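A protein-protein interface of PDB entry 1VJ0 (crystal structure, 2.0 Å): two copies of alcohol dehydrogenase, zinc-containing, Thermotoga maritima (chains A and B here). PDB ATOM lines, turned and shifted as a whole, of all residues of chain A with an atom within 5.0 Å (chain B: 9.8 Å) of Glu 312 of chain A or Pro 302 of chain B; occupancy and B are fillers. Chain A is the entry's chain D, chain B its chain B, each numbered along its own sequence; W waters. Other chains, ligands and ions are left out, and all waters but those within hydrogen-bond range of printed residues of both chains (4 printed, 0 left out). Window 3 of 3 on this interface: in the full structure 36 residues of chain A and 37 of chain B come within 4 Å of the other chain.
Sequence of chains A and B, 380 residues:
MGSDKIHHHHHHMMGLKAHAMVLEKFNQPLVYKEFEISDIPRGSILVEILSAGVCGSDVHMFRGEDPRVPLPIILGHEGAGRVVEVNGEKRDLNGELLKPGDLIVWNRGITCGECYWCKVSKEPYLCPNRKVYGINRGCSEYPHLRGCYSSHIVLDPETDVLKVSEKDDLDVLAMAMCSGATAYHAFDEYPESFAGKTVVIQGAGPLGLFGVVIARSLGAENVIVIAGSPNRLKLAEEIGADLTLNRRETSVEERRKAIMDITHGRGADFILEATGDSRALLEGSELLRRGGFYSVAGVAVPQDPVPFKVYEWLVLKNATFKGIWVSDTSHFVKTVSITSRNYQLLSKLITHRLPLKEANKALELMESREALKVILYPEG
CB of Val 310 of chain A touches OG of Ser 278 of chain B, 3.4 Å away.
Val 310 of chain A touches Val 296 of chain B.
Val 310 of chain A touches Val 299 of chain B.
Val 306 of chain B touches Val 310 of chain A (CG2 to CG2, 3.9 Å).
O of Val 299 of chain B touches CD1 of Tyr 311 of chain A, at 3.7 Å.
Tyr 311 of chain A touches Val 301 of chain B.
Tyr 311 of chain A touches Pro 302 of chain B.
Glu 312 of chain A touches Pro 302 of chain B.
Gly 323 of chain B touches Leu 314 of chain A (CA to O, 3.2 Å).
CH2 of Trp 325 of chain B touches CD1 of Leu 316 of chain A, 3.7 Å away.
Of the 18 printed residues of chain B, 9 touch a printed residue of chain A.
Printed residues of chain B that touch a printed residue of chain A: Ser 278, Val 296, Val 299, Ala 300, Val 301, Pro 302, Val 306, Gly 323 and Trp 325.
Hydrophobic or aromatic side chains of chain B within 4 Å of the printed part of chain A: Val 296, Val 299, Pro 302, Val 306 and Trp 325.
Along chain B the printed residues that touch a printed residue of chain A span positions 278 to 325.
Among the printed residues, 12 pairs touch across the chains.
Among the printed residues, no Asp or Glu carboxylate lies within 4 Å of a Lys or Arg side-chain nitrogen of the other chain.
Water W4 bridges the backbone carbonyl oxygen of Gln 303 of chain B (2.7 Å) and the side-chain carboxylate of Glu 312 of chain A (2.9 Å).
Water W3 bridges the backbone carbonyl oxygen (O) of Ala 300 of chain B (2.7 Å) and the side-chain hydroxyl (OH) of Tyr 311 of chain A (2.8 Å).
Water W1 lies within hydrogen-bond range of OE1 of Glu 312 of chain A, N of Gln 303 of chain B and N of Tyr 311 of chain A.
Water W2 lies within hydrogen-bond range of O of Asp 304 of chain B (2.7 Å), OG of Ser 278 of chain B (2.8 Å) and N of Val 310 of chain A (3.2 Å).
No position is printed for both chains.
O of Tyr 311 of chain A sits at hydrogen-bond distance from N of Leu 316 of chain A, 2.8 Å away.
OG of Ser 278 of chain B sits at hydrogen-bond distance from OE1 of Gln 303 of chain B.
Pro 302 of chain B touches two residues of chain A.
No residue of chain B comes within 4 Å of Lys 309 of chain A.
Tyr 311 of chain A touches five residues of chain B.
Printed residues of chain A within 4 Å of Trp 325 of chain B: Tyr 311 (3.6 Å) and Leu 316 (3.7 Å).
Of the printed residues of chain B, Leu 314 of chain A touches Gly 323.
Of the printed residues of chain B, Leu 316 of chain A touches Trp 325 (3.7 Å).
Of the printed residues of chain A, Gly 323 of chain B touches Leu 314.
Printed residues of chain A within 4 Å of Val 301 of chain B: Tyr 311.
The nearest printed residue of chain B that does not touch Val 310 of chain A is Pro 305 of chain B (5.5 Å).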
ATOM      1  N   LYS A 309      -1.431   7.360  30.352  1.00  0.00           N
ATOM      2  CA  LYS A 309      -1.148   8.672  29.807  1.00  0.00           C
ATOM      3  C   LYS A 309      -0.876   8.548  28.316  1.00  0.00           C
ATOM      4  O   LYS A 309       0.217   8.203  27.919  1.00  0.00           O
ATOM      5  CB  LYS A 309       0.077   9.261  30.497  1.00  0.00           C
ATOM      6  CG  LYS A 309      -0.148   9.552  31.961  1.00  0.00           C
ATOM      7  CD  LYS A 309       1.115  10.063  32.623  1.00  0.00           C
ATOM      8  CE  LYS A 309       0.744  10.590  34.008  1.00  0.00           C
ATOM      9  NZ  LYS A 309       1.941  10.841  34.813  1.00  0.00           N
ATOM     10  N   VAL A 310      -1.911   8.802  27.508  1.00  0.00           N
ATOM     11  CA  VAL A 310      -1.878   8.536  26.041  1.00  0.00           C
ATOM     12  C   VAL A 310      -0.883   9.444  25.325  1.00  0.00           C
ATOM     13  O   VAL A 310      -0.058   8.971  24.531  1.00  0.00           O
ATOM     14  CB  VAL A 310      -3.260   8.693  25.438  1.00  0.00           C
ATOM     15  CG1 VAL A 310      -3.227   8.478  23.941  1.00  0.00           C
ATOM     16  CG2 VAL A 310      -4.245   7.711  26.139  1.00  0.00           C
ATOM     17  N   TYR A 311      -0.918  10.720  25.639  1.00  0.00           N
ATOM     18  CA  TYR A 311      -0.018  11.657  24.982  1.00  0.00           C
ATOM     19  C   TYR A 311       1.405  11.353  25.373  1.00  0.00           C
ATOM     20  O   TYR A 311       2.266  11.195  24.507  1.00  0.00           O
ATOM     21  CB  TYR A 311      -0.338  13.087  25.341  1.00  0.00           C
ATOM     22  CG  TYR A 311       0.569  14.093  24.654  1.00  0.00           C
ATOM     23  CD1 TYR A 311       0.458  14.318  23.284  1.00  0.00           C
ATOM     24  CD2 TYR A 311       1.522  14.829  25.368  1.00  0.00           C
ATOM     25  CE1 TYR A 311       1.262  15.222  22.637  1.00  0.00           C
ATOM     26  CE2 TYR A 311       2.329  15.737  24.726  1.00  0.00           C
ATOM     27  CZ  TYR A 311       2.204  15.932  23.350  1.00  0.00           C
ATOM     28  OH  TYR A 311       2.976  16.866  22.661  1.00  0.00           O
ATOM     29  N   GLU A 312       1.661  11.261  26.679  1.00  0.00           N
ATOM     30  CA  GLU A 312       3.044  11.063  27.159  1.00  0.00           C
ATOM     31  C   GLU A 312       3.668   9.744  26.824  1.00  0.00           C
ATOM     32  O   GLU A 312       4.827   9.699  26.460  1.00  0.00           O
ATOM     33  CB  GLU A 312       3.127  11.242  28.681  1.00  0.00           C
ATOM     34  CG  GLU A 312       2.811  12.653  29.113  1.00  0.00           C
ATOM     35  CD  GLU A 312       1.332  12.886  29.373  1.00  0.00           C
ATOM     36  OE1 GLU A 312       0.427  12.203  28.813  1.00  0.00           O
ATOM     37  OE2 GLU A 312       1.067  13.776  30.178  1.00  0.00           O
ATOM     38  N   TRP A 313       2.940   8.655  27.001  1.00  0.00           N
ATOM     39  CA  TRP A 313       3.519   7.336  26.852  1.00  0.00           C
ATOM     40  C   TRP A 313       3.416   6.746  25.480  1.00  0.00           C
ATOM     41  O   TRP A 313       4.211   5.865  25.161  1.00  0.00           O
ATOM     42  CB  TRP A 313       2.847   6.379  27.804  1.00  0.00           C
ATOM     43  CG  TRP A 313       3.084   6.801  29.186  1.00  0.00           C
ATOM     44  CD1 TRP A 313       4.032   7.699  29.634  1.00  0.00           C
ATOM     45  CD2 TRP A 313       2.449   6.292  30.329  1.00  0.00           C
ATOM     46  NE1 TRP A 313       3.977   7.769  31.001  1.00  0.00           N
ATOM     47  CE2 TRP A 313       3.041   6.886  31.445  1.00  0.00           C
ATOM     48  CE3 TRP A 313       1.481   5.325  30.532  1.00  0.00           C
ATOM     49  CZ2 TRP A 313       2.604   6.647  32.720  1.00  0.00           C
ATOM     50  CZ3 TRP A 313       1.072   5.074  31.810  1.00  0.00           C
ATOM     51  CH2 TRP A 313       1.631   5.715  32.873  1.00  0.00           C
ATOM     52  N   LEU A 314       2.445   7.201  24.684  1.00  0.00           N
ATOM     53  CA  LEU A 314       2.249   6.658  23.356  1.00  0.00           C
ATOM     54  C   LEU A 314       2.582   7.657  22.258  1.00  0.00           C
ATOM     55  O   LEU A 314       3.504   7.419  21.498  1.00  0.00           O
ATOM     56  CB  LEU A 314       0.815   6.176  23.172  1.00  0.00           C
ATOM     57  CG  LEU A 314       0.425   4.732  23.218  1.00  0.00           C
ATOM     58  CD1 LEU A 314      -1.069   4.691  22.851  1.00  0.00           C
ATOM     59  CD2 LEU A 314       1.271   3.805  22.315  1.00  0.00           C
ATOM     60  N   LEU A 316       3.608  11.226  22.026  1.00  0.00           N
ATOM     61  CA  LEU A 316       4.896  11.955  22.145  1.00  0.00           C
ATOM     62  C   LEU A 316       6.116  11.040  22.067  1.00  0.00           C
ATOM     63  O   LEU A 316       7.124  11.409  21.500  1.00  0.00           O
ATOM     64  CB  LEU A 316       4.940  12.764  23.443  1.00  0.00           C
ATOM     65  CG  LEU A 316       6.025  13.817  23.684  1.00  0.00           C
ATOM     66  CD1 LEU A 316       6.050  14.764  22.522  1.00  0.00           C
ATOM     67  CD2 LEU A 316       5.729  14.634  24.983  1.00  0.00           C
ATOM     68  N   LYS A 317       6.021   9.841  22.624  1.00  0.00           N
ATOM     69  CA  LYS A 317       7.099   8.909  22.643  1.00  0.00           C
ATOM     70  C   LYS A 317       7.194   8.121  21.335  1.00  0.00           C
ATOM     71  O   LYS A 317       8.196   7.457  21.096  1.00  0.00           O
ATOM     72  CB  LYS A 317       6.874   7.938  23.827  1.00  0.00           C
ATOM     73  CG  LYS A 317       8.074   7.242  24.348  1.00  0.00           C
ATOM     74  CD  LYS A 317       7.838   6.412  25.617  1.00  0.00           C
ATOM     75  CE  LYS A 317       7.815   7.303  26.860  1.00  0.00           C
ATOM     76  NZ  LYS A 317       9.096   7.423  27.511  1.00  0.00           N
ATOM     77  N   GLU B  65      -0.671  28.069  24.445  1.00  0.00           N
ATOM     78  CA  GLU B  65      -0.781  26.725  25.035  1.00  0.00           C
ATOM     79  C   GLU B  65       0.366  25.783  24.634  1.00  0.00           C
ATOM     80  O   GLU B  65       0.508  24.680  25.165  1.00  0.00           O
ATOM     81  CB  GLU B  65      -2.161  26.153  24.680  1.00  0.00           C
ATOM     82  CG  GLU B  65      -3.261  26.990  25.335  1.00  0.00           C
ATOM     83  CD  GLU B  65      -4.679  26.729  24.841  1.00  0.00           C
ATOM     84  OE1 GLU B  65      -4.859  26.243  23.684  1.00  0.00           O
ATOM     85  OE2 GLU B  65      -5.621  27.060  25.634  1.00  0.00           O
ATOM     86  N   ASP B  66       1.202  26.226  23.708  1.00  0.00           N
ATOM     87  CA  ASP B  66       2.284  25.407  23.187  1.00  0.00           C
ATOM     88  C   ASP B  66       3.566  25.944  23.784  1.00  0.00           C
ATOM     89  O   ASP B  66       3.927  27.093  23.538  1.00  0.00           O
ATOM     90  CB  ASP B  66       2.316  25.498  21.661  1.00  0.00           C
ATOM     91  CG  ASP B  66       3.296  24.501  21.018  1.00  0.00           C
ATOM     92  OD1 ASP B  66       4.393  24.247  21.594  1.00  0.00           O
ATOM     93  OD2 ASP B  66       3.042  23.948  19.910  1.00  0.00           O
ATOM     94  N   PRO B  67       4.267  25.135  24.563  1.00  0.00           N
ATOM     95  CA  PRO B  67       5.464  25.617  25.264  1.00  0.00           C
ATOM     96  C   PRO B  67       6.717  25.817  24.350  1.00  0.00           C
ATOM     97  O   PRO B  67       7.652  26.509  24.746  1.00  0.00           O
ATOM     98  CB  PRO B  67       5.682  24.546  26.347  1.00  0.00           C
ATOM     99  CG  PRO B  67       5.194  23.277  25.713  1.00  0.00           C
ATOM    100  CD  PRO B  67       4.024  23.704  24.817  1.00  0.00           C
ATOM    101  N   GLY B 276      -8.231  13.509  18.884  1.00  0.00           N
ATOM    102  CA  GLY B 276      -7.582  14.450  19.823  1.00  0.00           C
ATOM    103  C   GLY B 276      -7.971  14.174  21.259  1.00  0.00           C
ATOM    104  O   GLY B 276      -7.563  14.891  22.145  1.00  0.00           O
ATOM    105  N   ASP B 277      -8.825  13.176  21.479  1.00  0.00           N
ATOM    106  CA  ASP B 277      -9.311  12.861  22.807  1.00  0.00           C
ATOM    107  C   ASP B 277      -8.820  11.469  23.186  1.00  0.00           C
ATOM    108  O   ASP B 277      -9.163  10.498  22.514  1.00  0.00           O
ATOM    109  CB  ASP B 277     -10.829  12.910  22.775  1.00  0.00           C
ATOM    110  CG  ASP B 277     -11.480  12.806  24.137  1.00  0.00           C
ATOM    111  OD1 ASP B 277     -10.889  12.298  25.108  1.00  0.00           O
ATOM    112  OD2 ASP B 277     -12.641  13.253  24.309  1.00  0.00           O
ATOM    113  N   SER B 278      -8.060  11.381  24.286  1.00  0.00           N
ATOM    114  CA  SER B 278      -7.518  10.108  24.826  1.00  0.00           C
ATOM    115  C   SER B 278      -8.596   9.073  25.081  1.00  0.00           C
ATOM    116  O   SER B 278      -8.357   7.902  24.966  1.00  0.00           O
ATOM    117  CB  SER B 278      -6.814  10.369  26.155  1.00  0.00           C
ATOM    118  OG  SER B 278      -5.599  11.072  26.045  1.00  0.00           O
ATOM    119  N   VAL B 296      -2.209   5.653  17.054  1.00  0.00           N
ATOM    120  CA  VAL B 296      -2.715   6.739  17.854  1.00  0.00           C
ATOM    121  C   VAL B 296      -1.958   8.034  17.477  1.00  0.00           C
ATOM    122  O   VAL B 296      -0.794   8.241  17.817  1.00  0.00           O
ATOM    123  CB  VAL B 296      -2.645   6.379  19.362  1.00  0.00           C
ATOM    124  CG1 VAL B 296      -3.237   7.571  20.200  1.00  0.00           C
ATOM    125  CG2 VAL B 296      -3.380   5.089  19.593  1.00  0.00           C
ATOM    126  N   GLY B 298      -3.925  11.371  17.129  1.00  0.00           N
ATOM    127  CA  GLY B 298      -4.687  12.571  17.223  1.00  0.00           C
ATOM    128  C   GLY B 298      -4.427  13.340  18.507  1.00  0.00           C
ATOM    129  O   GLY B 298      -4.377  14.561  18.495  1.00  0.00           O
ATOM    130  N   VAL B 299      -4.314  12.638  19.621  1.00  0.00           N
ATOM    131  CA  VAL B 299      -4.118  13.278  20.924  1.00  0.00           C
ATOM    132  C   VAL B 299      -2.848  14.129  20.811  1.00  0.00           C
ATOM    133  O   VAL B 299      -1.797  13.627  20.421  1.00  0.00           O
ATOM    134  CB  VAL B 299      -3.938  12.245  22.044  1.00  0.00           C
ATOM    135  CG1 VAL B 299      -3.489  12.898  23.304  1.00  0.00           C
ATOM    136  CG2 VAL B 299      -5.183  11.379  22.268  1.00  0.00           C
ATOM    137  N   ALA B 300      -2.933  15.411  21.169  1.00  0.00           N
ATOM    138  CA  ALA B 300      -1.865  16.350  20.848  1.00  0.00           C
ATOM    139  C   ALA B 300      -1.448  17.172  22.047  1.00  0.00           C
ATOM    140  O   ALA B 300      -0.566  17.994  21.933  1.00  0.00           O
ATOM    141  CB  ALA B 300      -2.256  17.260  19.619  1.00  0.00           C
ATOM    142  N   VAL B 301      -2.045  16.911  23.216  1.00  0.00           N
ATOM    143  CA  VAL B 301      -1.702  17.620  24.455  1.00  0.00           C
ATOM    144  C   VAL B 301      -1.820  16.634  25.566  1.00  0.00           C
ATOM    145  O   VAL B 301      -2.579  15.650  25.450  1.00  0.00           O
ATOM    146  CB  VAL B 301      -2.648  18.838  24.805  1.00  0.00           C
ATOM    147  CG1 VAL B 301      -2.440  20.000  23.826  1.00  0.00           C
ATOM    148  CG2 VAL B 301      -4.071  18.421  24.849  1.00  0.00           C
ATOM    149  N   PRO B 302      -1.080  16.876  26.648  1.00  0.00           N
ATOM    150  CA  PRO B 302      -1.216  16.077  27.852  1.00  0.00           C
ATOM    151  C   PRO B 302      -2.666  16.125  28.325  1.00  0.00           C
ATOM    152  O   PRO B 302      -3.215  17.190  28.413  1.00  0.00           O
ATOM    153  CB  PRO B 302      -0.317  16.809  28.846  1.00  0.00           C
ATOM    154  CG  PRO B 302       0.640  17.585  27.974  1.00  0.00           C
ATOM    155  CD  PRO B 302      -0.071  17.953  26.799  1.00  0.00           C
ATOM    156  N   GLN B 303      -3.254  14.968  28.608  1.00  0.00           N
ATOM    157  CA  GLN B 303      -4.640  14.856  29.054  1.00  0.00           C
ATOM    158  C   GLN B 303      -4.702  14.011  30.311  1.00  0.00           C
ATOM    159  O   GLN B 303      -3.731  13.374  30.660  1.00  0.00           O
ATOM    160  CB  GLN B 303      -5.463  14.224  27.919  1.00  0.00           C
ATOM    161  CG  GLN B 303      -5.595  15.202  26.764  1.00  0.00           C
ATOM    162  CD  GLN B 303      -6.425  14.692  25.617  1.00  0.00           C
ATOM    163  OE1 GLN B 303      -6.609  13.499  25.431  1.00  0.00           O
ATOM    164  NE2 GLN B 303      -6.906  15.610  24.833  1.00  0.00           N
ATOM    165  N   ASP B 304      -5.852  13.978  30.980  1.00  0.00           N
ATOM    166  CA  ASP B 304      -6.044  13.046  32.108  1.00  0.00           C
ATOM    167  C   ASP B 304      -5.776  11.608  31.582  1.00  0.00           C
ATOM    168  O   ASP B 304      -6.092  11.310  30.434  1.00  0.00           O
ATOM    169  CB  ASP B 304      -7.455  13.113  32.654  1.00  0.00           C
ATOM    170  CG  ASP B 304      -7.762  14.408  33.343  1.00  0.00           C
ATOM    171  OD1 ASP B 304      -6.852  15.103  33.821  1.00  0.00           O
ATOM    172  OD2 ASP B 304      -8.920  14.821  33.464  1.00  0.00           O
ATOM    173  N   PRO B 305      -5.155  10.751  32.388  1.00  0.00           N
ATOM    174  CA  PRO B 305      -5.026   9.342  32.041  1.00  0.00           C
ATOM    175  C   PRO B 305      -6.385   8.664  31.825  1.00  0.00           C
ATOM    176  O   PRO B 305      -7.335   9.021  32.467  1.00  0.00           O
ATOM    177  CB  PRO B 305      -4.354   8.711  33.275  1.00  0.00           C
ATOM    178  CG  PRO B 305      -3.999   9.784  34.175  1.00  0.00           C
ATOM    179  CD  PRO B 305      -4.543  11.071  33.687  1.00  0.00           C
ATOM    180  N   VAL B 306      -6.431   7.681  30.950  1.00  0.00           N
ATOM    181  CA  VAL B 306      -7.625   6.885  30.736  1.00  0.00           C
ATOM    182  C   VAL B 306      -7.480   5.520  31.383  1.00  0.00           C
ATOM    183  O   VAL B 306      -6.372   4.992  31.446  1.00  0.00           O
ATOM    184  CB  VAL B 306      -7.922   6.726  29.246  1.00  0.00           C
ATOM    185  CG1 VAL B 306      -8.193   8.126  28.637  1.00  0.00           C
ATOM    186  CG2 VAL B 306      -6.862   5.951  28.490  1.00  0.00           C
ATOM    187  N   GLY B 323       1.903   4.759  18.974  1.00  0.00           N
ATOM    188  CA  GLY B 323       1.822   6.196  19.004  1.00  0.00           C
ATOM    189  C   GLY B 323       2.569   6.777  17.760  1.00  0.00           C
ATOM    190  O   GLY B 323       3.646   6.284  17.362  1.00  0.00           O
ATOM    191  N   TRP B 325       4.199  10.270  16.211  1.00  0.00           N
ATOM    192  CA  TRP B 325       4.692  11.622  16.400  1.00  0.00           C
ATOM    193  C   TRP B 325       5.097  12.258  15.062  1.00  0.00           C
ATOM    194  O   TRP B 325       6.060  11.823  14.412  1.00  0.00           O
ATOM    195  CB  TRP B 325       5.872  11.658  17.373  1.00  0.00           C
ATOM    196  CG  TRP B 325       6.323  13.031  17.684  1.00  0.00           C
ATOM    197  CD1 TRP B 325       7.501  13.605  17.307  1.00  0.00           C
ATOM    198  CD2 TRP B 325       5.583  14.037  18.363  1.00  0.00           C
ATOM    199  NE1 TRP B 325       7.557  14.897  17.744  1.00  0.00           N
ATOM    200  CE2 TRP B 325       6.373  15.203  18.367  1.00  0.00           C
ATOM    201  CE3 TRP B 325       4.296  14.086  18.955  1.00  0.00           C
ATOM    202  CZ2 TRP B 325       5.947  16.402  18.961  1.00  0.00           C
ATOM    203  CZ3 TRP B 325       3.863  15.305  19.527  1.00  0.00           C
ATOM    204  CH2 TRP B 325       4.681  16.425  19.526  1.00  0.00           C
HETATM  205  O   HOH W   1      -2.182  12.256  28.075  1.00  0.00           O
HETATM  206  O   HOH W   2      -4.361  10.552  28.487  1.00  0.00           O
HETATM  207  O   HOH W   3       1.665  17.893  20.440  1.00  0.00           O
HETATM  208  O   HOH W   4      -1.269  13.106  31.694  1.00  0.00           O
